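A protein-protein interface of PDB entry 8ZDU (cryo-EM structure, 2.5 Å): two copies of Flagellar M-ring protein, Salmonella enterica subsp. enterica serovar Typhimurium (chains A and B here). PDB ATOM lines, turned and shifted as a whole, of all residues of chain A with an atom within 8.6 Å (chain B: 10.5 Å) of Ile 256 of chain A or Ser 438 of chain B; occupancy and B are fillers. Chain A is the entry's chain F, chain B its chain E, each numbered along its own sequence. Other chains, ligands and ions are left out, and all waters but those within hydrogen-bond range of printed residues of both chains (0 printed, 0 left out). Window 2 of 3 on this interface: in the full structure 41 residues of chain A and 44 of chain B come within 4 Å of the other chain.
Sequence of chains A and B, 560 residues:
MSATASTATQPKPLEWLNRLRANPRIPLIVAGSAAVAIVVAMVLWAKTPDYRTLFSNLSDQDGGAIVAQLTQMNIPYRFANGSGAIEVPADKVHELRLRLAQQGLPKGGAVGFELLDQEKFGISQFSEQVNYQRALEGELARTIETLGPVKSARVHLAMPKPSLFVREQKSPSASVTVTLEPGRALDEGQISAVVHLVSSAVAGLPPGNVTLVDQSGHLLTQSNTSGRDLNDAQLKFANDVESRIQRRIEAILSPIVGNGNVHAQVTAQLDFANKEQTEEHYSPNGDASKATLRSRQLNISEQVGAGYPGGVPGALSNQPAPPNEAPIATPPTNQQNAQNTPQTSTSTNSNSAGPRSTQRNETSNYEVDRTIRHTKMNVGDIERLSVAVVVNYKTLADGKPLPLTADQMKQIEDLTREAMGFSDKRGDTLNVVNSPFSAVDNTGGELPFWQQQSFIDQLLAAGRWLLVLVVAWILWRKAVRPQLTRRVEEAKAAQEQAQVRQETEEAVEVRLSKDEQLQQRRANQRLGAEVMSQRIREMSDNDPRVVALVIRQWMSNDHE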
ATOM      1  N   GLU A 250      19.460 -27.396  33.431  1.00  0.00           N
ATOM      2  CA  GLU A 250      19.586 -28.439  32.419  1.00  0.00           C
ATOM      3  C   GLU A 250      18.227 -29.009  32.039  1.00  0.00           C
ATOM      4  O   GLU A 250      17.956 -29.253  30.858  1.00  0.00           O
ATOM      5  CB  GLU A 250      20.516 -29.546  32.917  1.00  0.00           C
ATOM      6  CG  GLU A 250      21.952 -29.403  32.442  1.00  0.00           C
ATOM      7  CD  GLU A 250      22.949 -30.040  33.390  1.00  0.00           C
ATOM      8  OE1 GLU A 250      22.514 -30.658  34.385  1.00  0.00           O
ATOM      9  OE2 GLU A 250      24.167 -29.923  33.140  1.00  0.00           O
ATOM     10  N   ALA A 251      17.353 -29.223  33.027  1.00  0.00           N
ATOM     11  CA  ALA A 251      16.029 -29.760  32.739  1.00  0.00           C
ATOM     12  C   ALA A 251      15.206 -28.791  31.900  1.00  0.00           C
ATOM     13  O   ALA A 251      14.502 -29.209  30.973  1.00  0.00           O
ATOM     14  CB  ALA A 251      15.302 -30.094  34.042  1.00  0.00           C
ATOM     15  N   ILE A 252      15.271 -27.493  32.210  1.00  0.00           N
ATOM     16  CA  ILE A 252      14.457 -26.547  31.453  1.00  0.00           C
ATOM     17  C   ILE A 252      15.013 -26.347  30.044  1.00  0.00           C
ATOM     18  O   ILE A 252      14.244 -26.163  29.093  1.00  0.00           O
ATOM     19  CB  ILE A 252      14.313 -25.209  32.209  1.00  0.00           C
ATOM     20  CG1 ILE A 252      13.322 -24.294  31.488  1.00  0.00           C
ATOM     21  CG2 ILE A 252      15.646 -24.505  32.354  1.00  0.00           C
ATOM     22  CD1 ILE A 252      11.948 -24.903  31.306  1.00  0.00           C
ATOM     23  N   LEU A 253      16.337 -26.386  29.873  1.00  0.00           N
ATOM     24  CA  LEU A 253      16.930 -26.126  28.567  1.00  0.00           C
ATOM     25  C   LEU A 253      17.063 -27.368  27.692  1.00  0.00           C
ATOM     26  O   LEU A 253      17.331 -27.232  26.494  1.00  0.00           O
ATOM     27  CB  LEU A 253      18.309 -25.479  28.736  1.00  0.00           C
ATOM     28  CG  LEU A 253      18.344 -23.951  28.681  1.00  0.00           C
ATOM     29  CD1 LEU A 253      19.774 -23.444  28.756  1.00  0.00           C
ATOM     30  CD2 LEU A 253      17.655 -23.443  27.424  1.00  0.00           C
ATOM     31  N   SER A 254      16.890 -28.565  28.253  1.00  0.00           N
ATOM     32  CA  SER A 254      17.087 -29.788  27.473  1.00  0.00           C
ATOM     33  C   SER A 254      16.111 -29.945  26.311  1.00  0.00           C
ATOM     34  O   SER A 254      16.567 -30.256  25.197  1.00  0.00           O
ATOM     35  CB  SER A 254      17.032 -31.001  28.408  1.00  0.00           C
ATOM     36  OG  SER A 254      18.332 -31.376  28.835  1.00  0.00           O
ATOM     37  N   PRO A 255      14.793 -29.772  26.478  1.00  0.00           N
ATOM     38  CA  PRO A 255      13.873 -30.114  25.378  1.00  0.00           C
ATOM     39  C   PRO A 255      14.111 -29.346  24.087  1.00  0.00           C
ATOM     40  O   PRO A 255      13.886 -29.901  23.004  1.00  0.00           O
ATOM     41  CB  PRO A 255      12.499 -29.788  25.977  1.00  0.00           C
ATOM     42  CG  PRO A 255      12.693 -30.037  27.428  1.00  0.00           C
ATOM     43  CD  PRO A 255      14.033 -29.408  27.689  1.00  0.00           C
ATOM     44  N   ILE A 256      14.555 -28.093  24.159  1.00  0.00           N
ATOM     45  CA  ILE A 256      14.632 -27.263  22.957  1.00  0.00           C
ATOM     46  C   ILE A 256      15.908 -27.551  22.174  1.00  0.00           C
ATOM     47  O   ILE A 256      15.862 -27.994  21.021  1.00  0.00           O
ATOM     48  CB  ILE A 256      14.523 -25.773  23.326  1.00  0.00           C
ATOM     49  CG1 ILE A 256      13.144 -25.471  23.914  1.00  0.00           C
ATOM     50  CG2 ILE A 256      14.785 -24.903  22.107  1.00  0.00           C
ATOM     51  CD1 ILE A 256      13.030 -24.093  24.516  1.00  0.00           C
ATOM     52  N   VAL A 257      17.066 -27.300  22.788  1.00  0.00           N
ATOM     53  CA  VAL A 257      18.327 -27.389  22.055  1.00  0.00           C
ATOM     54  C   VAL A 257      18.691 -28.844  21.772  1.00  0.00           C
ATOM     55  O   VAL A 257      19.287 -29.159  20.736  1.00  0.00           O
ATOM     56  CB  VAL A 257      19.446 -26.645  22.811  1.00  0.00           C
ATOM     57  CG1 VAL A 257      18.942 -25.294  23.296  1.00  0.00           C
ATOM     58  CG2 VAL A 257      19.967 -27.464  23.984  1.00  0.00           C
ATOM     59  N   GLY A 258      18.342 -29.743  22.675  1.00  0.00           N
ATOM     60  CA  GLY A 258      18.683 -31.144  22.516  1.00  0.00           C
ATOM     61  C   GLY A 258      19.027 -31.772  23.849  1.00  0.00           C
ATOM     62  O   GLY A 258      19.216 -31.096  24.859  1.00  0.00           O
ATOM     63  N   ASN A 259      19.113 -33.104  23.832  1.00  0.00           N
ATOM     64  CA  ASN A 259      19.360 -33.847  25.063  1.00  0.00           C
ATOM     65  C   ASN A 259      20.736 -33.539  25.642  1.00  0.00           C
ATOM     66  O   ASN A 259      20.875 -33.351  26.856  1.00  0.00           O
ATOM     67  CB  ASN A 259      19.210 -35.347  24.809  1.00  0.00           C
ATOM     68  CG  ASN A 259      18.504 -36.062  25.943  1.00  0.00           C
ATOM     69  OD1 ASN A 259      19.081 -36.283  27.007  1.00  0.00           O
ATOM     70  ND2 ASN A 259      17.246 -36.427  25.721  1.00  0.00           N
ATOM     71  N   GLY A 260      21.762 -33.484  24.796  1.00  0.00           N
ATOM     72  CA  GLY A 260      23.112 -33.273  25.281  1.00  0.00           C
ATOM     73  C   GLY A 260      23.873 -32.180  24.560  1.00  0.00           C
ATOM     74  O   GLY A 260      25.088 -32.287  24.367  1.00  0.00           O
ATOM     75  N   ASN A 261      23.172 -31.122  24.152  1.00  0.00           N
ATOM     76  CA  ASN A 261      23.779 -29.998  23.450  1.00  0.00           C
ATOM     77  C   ASN A 261      23.839 -28.744  24.318  1.00  0.00           C
ATOM     78  O   ASN A 261      23.817 -27.625  23.801  1.00  0.00           O
ATOM     79  CB  ASN A 261      23.025 -29.703  22.153  1.00  0.00           C
ATOM     80  CG  ASN A 261      22.931 -30.912  21.240  1.00  0.00           C
ATOM     81  OD1 ASN A 261      23.050 -32.052  21.683  1.00  0.00           O
ATOM     82  ND2 ASN A 261      22.718 -30.662  19.953  1.00  0.00           N
ATOM     83  N   VAL A 262      23.916 -28.912  25.636  1.00  0.00           N
ATOM     84  CA  VAL A 262      23.937 -27.774  26.547  1.00  0.00           C
ATOM     85  C   VAL A 262      24.650 -28.189  27.827  1.00  0.00           C
ATOM     86  O   VAL A 262      24.502 -29.320  28.301  1.00  0.00           O
ATOM     87  CB  VAL A 262      22.503 -27.256  26.824  1.00  0.00           C
ATOM     88  CG1 VAL A 262      21.643 -28.345  27.451  1.00  0.00           C
ATOM     89  CG2 VAL A 262      22.536 -26.014  27.705  1.00  0.00           C
ATOM     90  N   LYS A 394      23.809 -25.785  15.578  1.00  0.00           N
ATOM     91  CA  LYS A 394      22.741 -26.571  14.970  1.00  0.00           C
ATOM     92  C   LYS A 394      23.305 -27.306  13.760  1.00  0.00           C
ATOM     93  O   LYS A 394      23.799 -26.679  12.817  1.00  0.00           O
ATOM     94  CB  LYS A 394      21.567 -25.677  14.577  1.00  0.00           C
ATOM     95  CG  LYS A 394      20.470 -26.390  13.796  1.00  0.00           C
ATOM     96  CD  LYS A 394      19.947 -27.613  14.538  1.00  0.00           C
ATOM     97  CE  LYS A 394      19.303 -27.232  15.863  1.00  0.00           C
ATOM     98  NZ  LYS A 394      19.060 -28.423  16.724  1.00  0.00           N
ATOM     99  N   LEU A 404      23.053 -20.657  15.720  1.00  0.00           N
ATOM    100  CA  LEU A 404      21.659 -20.455  16.081  1.00  0.00           C
ATOM    101  C   LEU A 404      21.237 -19.012  15.830  1.00  0.00           C
ATOM    102  O   LEU A 404      22.058 -18.092  15.814  1.00  0.00           O
ATOM    103  CB  LEU A 404      21.426 -20.817  17.549  1.00  0.00           C
ATOM    104  CG  LEU A 404      20.786 -22.182  17.815  1.00  0.00           C
ATOM    105  CD1 LEU A 404      21.815 -23.294  17.688  1.00  0.00           C
ATOM    106  CD2 LEU A 404      20.130 -22.208  19.187  1.00  0.00           C
ATOM    107  N   GLN A 408      16.468 -17.278  18.989  1.00  0.00           N
ATOM    108  CA  GLN A 408      16.645 -18.479  19.799  1.00  0.00           C
ATOM    109  C   GLN A 408      17.572 -18.211  20.978  1.00  0.00           C
ATOM    110  O   GLN A 408      17.322 -18.684  22.094  1.00  0.00           O
ATOM    111  CB  GLN A 408      17.183 -19.620  18.935  1.00  0.00           C
ATOM    112  CG  GLN A 408      16.105 -20.420  18.225  1.00  0.00           C
ATOM    113  CD  GLN A 408      16.670 -21.360  17.179  1.00  0.00           C
ATOM    114  OE1 GLN A 408      17.278 -20.927  16.201  1.00  0.00           O
ATOM    115  NE2 GLN A 408      16.471 -22.658  17.382  1.00  0.00           N
ATOM    116  N   MET A 409      18.645 -17.451  20.750  1.00  0.00           N
ATOM    117  CA  MET A 409      19.543 -17.093  21.844  1.00  0.00           C
ATOM    118  C   MET A 409      18.831 -16.249  22.893  1.00  0.00           C
ATOM    119  O   MET A 409      19.026 -16.449  24.096  1.00  0.00           O
ATOM    120  CB  MET A 409      20.766 -16.353  21.302  1.00  0.00           C
ATOM    121  CG  MET A 409      21.594 -17.164  20.325  1.00  0.00           C
ATOM    122  SD  MET A 409      21.921 -18.821  20.949  1.00  0.00           S
ATOM    123  CE  MET A 409      23.110 -18.461  22.239  1.00  0.00           C
ATOM    124  N   GLN A 411      15.608 -16.262  23.575  1.00  0.00           N
ATOM    125  CA  GLN A 411      14.708 -17.153  24.300  1.00  0.00           C
ATOM    126  C   GLN A 411      15.469 -18.009  25.305  1.00  0.00           C
ATOM    127  O   GLN A 411      15.000 -18.226  26.430  1.00  0.00           O
ATOM    128  CB  GLN A 411      13.936 -18.034  23.317  1.00  0.00           C
ATOM    129  CG  GLN A 411      12.960 -17.270  22.436  1.00  0.00           C
ATOM    130  CD  GLN A 411      12.288 -18.155  21.405  1.00  0.00           C
ATOM    131  OE1 GLN A 411      12.815 -19.204  21.033  1.00  0.00           O
ATOM    132  NE2 GLN A 411      11.120 -17.735  20.936  1.00  0.00           N
ATOM    133  N   ILE A 412      16.646 -18.508  24.916  1.00  0.00           N
ATOM    134  CA  ILE A 412      17.452 -19.317  25.826  1.00  0.00           C
ATOM    135  C   ILE A 412      17.893 -18.492  27.030  1.00  0.00           C
ATOM    136  O   ILE A 412      17.848 -18.964  28.175  1.00  0.00           O
ATOM    137  CB  ILE A 412      18.655 -19.923  25.077  1.00  0.00           C
ATOM    138  CG1 ILE A 412      18.204 -21.102  24.213  1.00  0.00           C
ATOM    139  CG2 ILE A 412      19.736 -20.363  26.053  1.00  0.00           C
ATOM    140  CD1 ILE A 412      19.100 -21.367  23.025  1.00  0.00           C
ATOM    141  N   LEU A 415      14.892 -18.032  29.335  1.00  0.00           N
ATOM    142  CA  LEU A 415      14.589 -19.252  30.078  1.00  0.00           C
ATOM    143  C   LEU A 415      15.604 -19.492  31.189  1.00  0.00           C
ATOM    144  O   LEU A 415      15.236 -19.892  32.300  1.00  0.00           O
ATOM    145  CB  LEU A 415      14.536 -20.447  29.128  1.00  0.00           C
ATOM    146  CG  LEU A 415      13.366 -20.468  28.143  1.00  0.00           C
ATOM    147  CD1 LEU A 415      13.494 -21.640  27.187  1.00  0.00           C
ATOM    148  CD2 LEU A 415      12.039 -20.518  28.884  1.00  0.00           C
ATOM    149  N   GLY B 260       1.986 -34.624  26.445  1.00  0.00           N
ATOM    150  CA  GLY B 260       3.404 -34.420  26.672  1.00  0.00           C
ATOM    151  C   GLY B 260       4.027 -33.342  25.810  1.00  0.00           C
ATOM    152  O   GLY B 260       5.185 -33.462  25.399  1.00  0.00           O
ATOM    153  N   ASN B 261       3.270 -32.282  25.525  1.00  0.00           N
ATOM    154  CA  ASN B 261       3.745 -31.171  24.710  1.00  0.00           C
ATOM    155  C   ASN B 261       3.973 -29.909  25.538  1.00  0.00           C
ATOM    156  O   ASN B 261       3.863 -28.795  25.020  1.00  0.00           O
ATOM    157  CB  ASN B 261       2.769 -30.883  23.570  1.00  0.00           C
ATOM    158  CG  ASN B 261       2.502 -32.100  22.703  1.00  0.00           C
ATOM    159  OD1 ASN B 261       2.692 -33.237  23.132  1.00  0.00           O
ATOM    160  ND2 ASN B 261       2.057 -31.863  21.476  1.00  0.00           N
ATOM    161  N   VAL B 262       4.289 -30.064  26.820  1.00  0.00           N
ATOM    162  CA  VAL B 262       4.483 -28.916  27.700  1.00  0.00           C
ATOM    163  C   VAL B 262       5.417 -29.324  28.831  1.00  0.00           C
ATOM    164  O   VAL B 262       5.351 -30.449  29.338  1.00  0.00           O
ATOM    165  CB  VAL B 262       3.128 -28.382  28.228  1.00  0.00           C
ATOM    166  CG1 VAL B 262       2.391 -29.458  29.014  1.00  0.00           C
ATOM    167  CG2 VAL B 262       3.331 -27.132  29.073  1.00  0.00           C
ATOM    168  N   HIS B 263       6.303 -28.404  29.209  1.00  0.00           N
ATOM    169  CA  HIS B 263       7.194 -28.583  30.347  1.00  0.00           C
ATOM    170  C   HIS B 263       7.278 -27.273  31.114  1.00  0.00           C
ATOM    171  O   HIS B 263       7.129 -26.191  30.541  1.00  0.00           O
ATOM    172  CB  HIS B 263       8.597 -29.027  29.911  1.00  0.00           C
ATOM    173  CG  HIS B 263       8.612 -30.293  29.113  1.00  0.00           C
ATOM    174  ND1 HIS B 263       8.574 -31.542  29.697  1.00  0.00           N
ATOM    175  CD2 HIS B 263       8.665 -30.505  27.776  1.00  0.00           C
ATOM    176  CE1 HIS B 263       8.600 -32.468  28.754  1.00  0.00           C
ATOM    177  NE2 HIS B 263       8.656 -31.865  27.580  1.00  0.00           N
ATOM    178  N   ALA B 264       7.517 -27.378  32.421  1.00  0.00           N
ATOM    179  CA  ALA B 264       7.596 -26.206  33.280  1.00  0.00           C
ATOM    180  C   ALA B 264       8.619 -26.438  34.382  1.00  0.00           C
ATOM    181  O   ALA B 264       8.880 -27.576  34.780  1.00  0.00           O
ATOM    182  CB  ALA B 264       6.232 -25.865  33.896  1.00  0.00           C
ATOM    183  N   ALA B 388       9.018 -20.644  34.351  1.00  0.00           N
ATOM    184  CA  ALA B 388       9.333 -20.756  32.934  1.00  0.00           C
ATOM    185  C   ALA B 388       8.553 -21.921  32.344  1.00  0.00           C
ATOM    186  O   ALA B 388       8.560 -23.024  32.901  1.00  0.00           O
ATOM    187  CB  ALA B 388      10.834 -20.959  32.713  1.00  0.00           C
ATOM    188  N   VAL B 389       7.882 -21.675  31.221  1.00  0.00           N
ATOM    189  CA  VAL B 389       7.061 -22.675  30.551  1.00  0.00           C
ATOM    190  C   VAL B 389       7.484 -22.749  29.091  1.00  0.00           C
ATOM    191  O   VAL B 389       7.716 -21.719  28.450  1.00  0.00           O
ATOM    192  CB  VAL B 389       5.556 -22.348  30.665  1.00  0.00           C
ATOM    193  CG1 VAL B 389       4.721 -23.404  29.955  1.00  0.00           C
ATOM    194  CG2 VAL B 389       5.142 -22.230  32.125  1.00  0.00           C
ATOM    195  N   VAL B 390       7.605 -23.970  28.572  1.00  0.00           N
ATOM    196  CA  VAL B 390       7.940 -24.206  27.173  1.00  0.00           C
ATOM    197  C   VAL B 390       6.862 -25.094  26.565  1.00  0.00           C
ATOM    198  O   VAL B 390       6.512 -26.133  27.134  1.00  0.00           O
ATOM    199  CB  VAL B 390       9.336 -24.845  27.017  1.00  0.00           C
ATOM    200  CG1 VAL B 390       9.511 -26.009  27.983  1.00  0.00           C
ATOM    201  CG2 VAL B 390       9.561 -25.296  25.582  1.00  0.00           C
ATOM    202  N   VAL B 391       6.328 -24.677  25.419  1.00  0.00           N
ATOM    203  CA  VAL B 391       5.269 -25.418  24.745  1.00  0.00           C
ATOM    204  C   VAL B 391       5.730 -25.793  23.344  1.00  0.00           C
ATOM    205  O   VAL B 391       6.567 -25.116  22.738  1.00  0.00           O
ATOM    206  CB  VAL B 391       3.944 -24.626  24.693  1.00  0.00           C
ATOM    207  CG1 VAL B 391       3.301 -24.580  26.071  1.00  0.00           C
ATOM    208  CG2 VAL B 391       4.181 -23.223  24.169  1.00  0.00           C
ATOM    209  N   ASN B 392       5.171 -26.885  22.831  1.00  0.00           N
ATOM    210  CA  ASN B 392       5.550 -27.443  21.543  1.00  0.00           C
ATOM    211  C   ASN B 392       4.707 -26.842  20.421  1.00  0.00           C
ATOM    212  O   ASN B 392       3.650 -26.249  20.647  1.00  0.00           O
ATOM    213  CB  ASN B 392       5.395 -28.966  21.558  1.00  0.00           C
ATOM    214  CG  ASN B 392       6.129 -29.644  20.414  1.00  0.00           C
ATOM    215  OD1 ASN B 392       6.529 -29.001  19.444  1.00  0.00           O
ATOM    216  ND2 ASN B 392       6.301 -30.957  20.521  1.00  0.00           N
ATOM    217  N   TYR B 393       5.197 -27.006  19.194  1.00  0.00           N
ATOM    218  CA  TYR B 393       4.462 -26.574  18.017  1.00  0.00           C
ATOM    219  C   TYR B 393       3.296 -27.518  17.736  1.00  0.00           C
ATOM    220  O   TYR B 393       3.234 -28.644  18.237  1.00  0.00           O
ATOM    221  CB  TYR B 393       5.385 -26.514  16.799  1.00  0.00           C
ATOM    222  CG  TYR B 393       5.963 -25.145  16.519  1.00  0.00           C
ATOM    223  CD1 TYR B 393       5.995 -24.167  17.504  1.00  0.00           C
ATOM    224  CD2 TYR B 393       6.476 -24.831  15.268  1.00  0.00           C
ATOM    225  CE1 TYR B 393       6.523 -22.915  17.249  1.00  0.00           C
ATOM    226  CE2 TYR B 393       7.005 -23.582  15.005  1.00  0.00           C
ATOM    227  CZ  TYR B 393       7.026 -22.628  15.998  1.00  0.00           C
ATOM    228  OH  TYR B 393       7.552 -21.384  15.740  1.00  0.00           O
ATOM    229  N   THR B 395       1.446 -29.903  15.293  1.00  0.00           N
ATOM    230  CA  THR B 395       1.733 -30.754  14.148  1.00  0.00           C
ATOM    231  C   THR B 395       0.438 -31.323  13.583  1.00  0.00           C
ATOM    232  O   THR B 395      -0.388 -31.868  14.320  1.00  0.00           O
ATOM    233  CB  THR B 395       2.675 -31.895  14.536  1.00  0.00           C
ATOM    234  OG1 THR B 395       2.070 -32.690  15.563  1.00  0.00           O
ATOM    235  CG2 THR B 395       3.998 -31.342  15.046  1.00  0.00           C
ATOM    236  N   ASN B 431       7.420 -16.502  32.358  1.00  0.00           N
ATOM    237  CA  ASN B 431       7.841 -16.443  30.963  1.00  0.00           C
ATOM    238  C   ASN B 431       7.427 -17.724  30.256  1.00  0.00           C
ATOM    239  O   ASN B 431       7.704 -18.822  30.746  1.00  0.00           O
ATOM    240  CB  ASN B 431       9.355 -16.240  30.848  1.00  0.00           C
ATOM    241  CG  ASN B 431       9.766 -15.657  29.510  1.00  0.00           C
ATOM    242  OD1 ASN B 431      10.050 -14.464  29.401  1.00  0.00           O
ATOM    243  ND2 ASN B 431       9.801 -16.497  28.483  1.00  0.00           N
ATOM    244  N   VAL B 432       6.770 -17.579  29.106  1.00  0.00           N
ATOM    245  CA  VAL B 432       6.287 -18.703  28.310  1.00  0.00           C
ATOM    246  C   VAL B 432       6.881 -18.590  26.912  1.00  0.00           C
ATOM    247  O   VAL B 432       6.841 -17.516  26.300  1.00  0.00           O
ATOM    248  CB  VAL B 432       4.748 -18.741  28.247  1.00  0.00           C
ATOM    249  CG1 VAL B 432       4.276 -20.030  27.595  1.00  0.00           C
ATOM    250  CG2 VAL B 432       4.154 -18.592  29.640  1.00  0.00           C
ATOM    251  N   VAL B 433       7.428 -19.697  26.411  1.00  0.00           N
ATOM    252  CA  VAL B 433       8.088 -19.741  25.112  1.00  0.00           C
ATOM    253  C   VAL B 433       7.514 -20.899  24.305  1.00  0.00           C
ATOM    254  O   VAL B 433       7.365 -22.015  24.818  1.00  0.00           O
ATOM    255  CB  VAL B 433       9.618 -19.886  25.258  1.00  0.00           C
ATOM    256  CG1 VAL B 433      10.273 -20.076  23.898  1.00  0.00           C
ATOM    257  CG2 VAL B 433      10.203 -18.675  25.967  1.00  0.00           C
ATOM    258  N   ASN B 434       7.197 -20.632  23.040  1.00  0.00           N
ATOM    259  CA  ASN B 434       6.708 -21.642  22.111  1.00  0.00           C
ATOM    260  C   ASN B 434       7.807 -21.947  21.103  1.00  0.00           C
ATOM    261  O   ASN B 434       8.278 -21.046  20.402  1.00  0.00           O
ATOM    262  CB  ASN B 434       5.438 -21.165  21.404  1.00  0.00           C
ATOM    263  CG  ASN B 434       4.895 -22.185  20.425  1.00  0.00           C
ATOM    264  OD1 ASN B 434       4.929 -23.389  20.680  1.00  0.00           O
ATOM    265  ND2 ASN B 434       4.378 -21.707  19.300  1.00  0.00           N
ATOM    266  N   SER B 435       8.211 -23.215  21.032  1.00  0.00           N
ATOM    267  CA  SER B 435       9.304 -23.629  20.162  1.00  0.00           C
ATOM    268  C   SER B 435       9.142 -25.109  19.855  1.00  0.00           C
ATOM    269  O   SER B 435       8.682 -25.867  20.717  1.00  0.00           O
ATOM    270  CB  SER B 435      10.665 -23.363  20.820  1.00  0.00           C
ATOM    271  OG  SER B 435      11.731 -23.595  19.916  1.00  0.00           O
ATOM    272  N   PRO B 436       9.495 -25.548  18.646  1.00  0.00           N
ATOM    273  CA  PRO B 436       9.384 -26.975  18.321  1.00  0.00           C
ATOM    274  C   PRO B 436      10.285 -27.823  19.207  1.00  0.00           C
ATOM    275  O   PRO B 436      11.403 -27.430  19.548  1.00  0.00           O
ATOM    276  CB  PRO B 436       9.814 -27.041  16.851  1.00  0.00           C
ATOM    277  CG  PRO B 436      10.606 -25.794  16.622  1.00  0.00           C
ATOM    278  CD  PRO B 436       9.994 -24.757  17.510  1.00  0.00           C
ATOM    279  N   PHE B 437       9.786 -28.998  19.577  1.00  0.00           N
ATOM    280  CA  PHE B 437      10.533 -29.906  20.433  1.00  0.00           C
ATOM    281  C   PHE B 437      11.580 -30.667  19.629  1.00  0.00           C
ATOM    282  O   PHE B 437      11.451 -30.856  18.416  1.00  0.00           O
ATOM    283  CB  PHE B 437       9.592 -30.893  21.125  1.00  0.00           C
ATOM    284  CG  PHE B 437       8.939 -30.345  22.364  1.00  0.00           C
ATOM    285  CD1 PHE B 437       8.911 -28.981  22.608  1.00  0.00           C
ATOM    286  CD2 PHE B 437       8.350 -31.195  23.285  1.00  0.00           C
ATOM    287  CE1 PHE B 437       8.310 -28.478  23.747  1.00  0.00           C
ATOM    288  CE2 PHE B 437       7.748 -30.698  24.425  1.00  0.00           C
ATOM    289  CZ  PHE B 437       7.728 -29.338  24.655  1.00  0.00           C
ATOM    290  N   SER B 438      12.625 -31.107  20.322  1.00  0.00           N
ATOM    291  CA  SER B 438      13.700 -31.864  19.691  1.00  0.00           C
ATOM    292  C   SER B 438      13.626 -33.339  20.071  1.00  0.00           C
ATOM    293  O   SER B 438      13.150 -34.167  19.294  1.00  0.00           O
ATOM    294  CB  SER B 438      15.063 -31.288  20.081  1.00  0.00           C
ATOM    295  OG  SER B 438      16.117 -32.042  19.505  1.00  0.00           O
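O of Val 433 of chain B is in hydrogen-bond range of N of Val 391 of chain B, 2.9 Å away. O of His 263 of chain B lies within hydrogen-bond range of N of Val 390 of chain B (3.0 Å). The backbone NH (N) of Ser 435 of chain B is in hydrogen-bond range of the backbone carbonyl oxygen (O) of Val 391 of chain B. The backbone NH (N) of Val 433 of chain B is in hydrogen-bond range of the backbone carbonyl oxygen (O) of Val 389 of chain B, at 2.9 Å.
Among the printed residues, pairs that only touch across the chains: Ile 256 of chain A with Val 390 of chain B, Ile 256 of chain A with Ser 435 of chain B, Ile 256 of chain A with Ser 438 of chain B, Gln 411 of chain A with Val 433 of chain B and Leu 415 of chain A with Val 433 of chain B.
Ile 256 of chain A touches just these residues of chain B: Val 390, Ser 435 and Ser 438. Ser 438 of chain B touches just these residues of chain A: Pro 255 (3.2 Å) and Ile 256 (3.5 Å). Of chain B, only Ser 438 comes within 4 Å of Pro 255 of chain A. No residue of chain B comes within 4 Å of Val 257 of chain A. No residue of chain B comes within 4 Å of Gly 258 of chain A. Printed residues of chain A within 4 Å of Val 433 of chain B: Gln 411 and Leu 415. Of the printed residues of chain A, Ser 435 of chain B touches Ile 256 (3.98 Å). Printed residues of chain B within 4 Å of Leu 415 of chain A: Val 433 (3.9 Å). Printed residues of chain A within 4 Å of Val 390 of chain B: Ile 256 (3.8 Å). Ala 251 of chain A touches none of the printed residues of chain B. The nearest residue of chain B that does not touch Ile 256 of chain A is Pro 436 of chain B (4.7 Å). The nearest residue of chain A that does not touch Ser 438 of chain B is Gly 258 of chain A (4.1 Å). The nearest printed residue of chain A that does not touch Val 390 of chain B is Ile 252 of chain A (4.3 Å).
3 positions are printed for both chains.
The backbone NH (N) of Ser 438 of chain B is in hydrogen-bond range of the backbone carbonyl oxygen (O) of Pro 255 of chain A.
Hydrophobic or aromatic side chains of chain A within 4 Å of the printed part of chain B: Ile 256 and Leu 415. Of the 20 printed residues of chain B, 4 touch a printed residue of chain A. Hydrophobic or aromatic side chains of chain B that line the printed part of chain A: Val 390 and Val 433.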
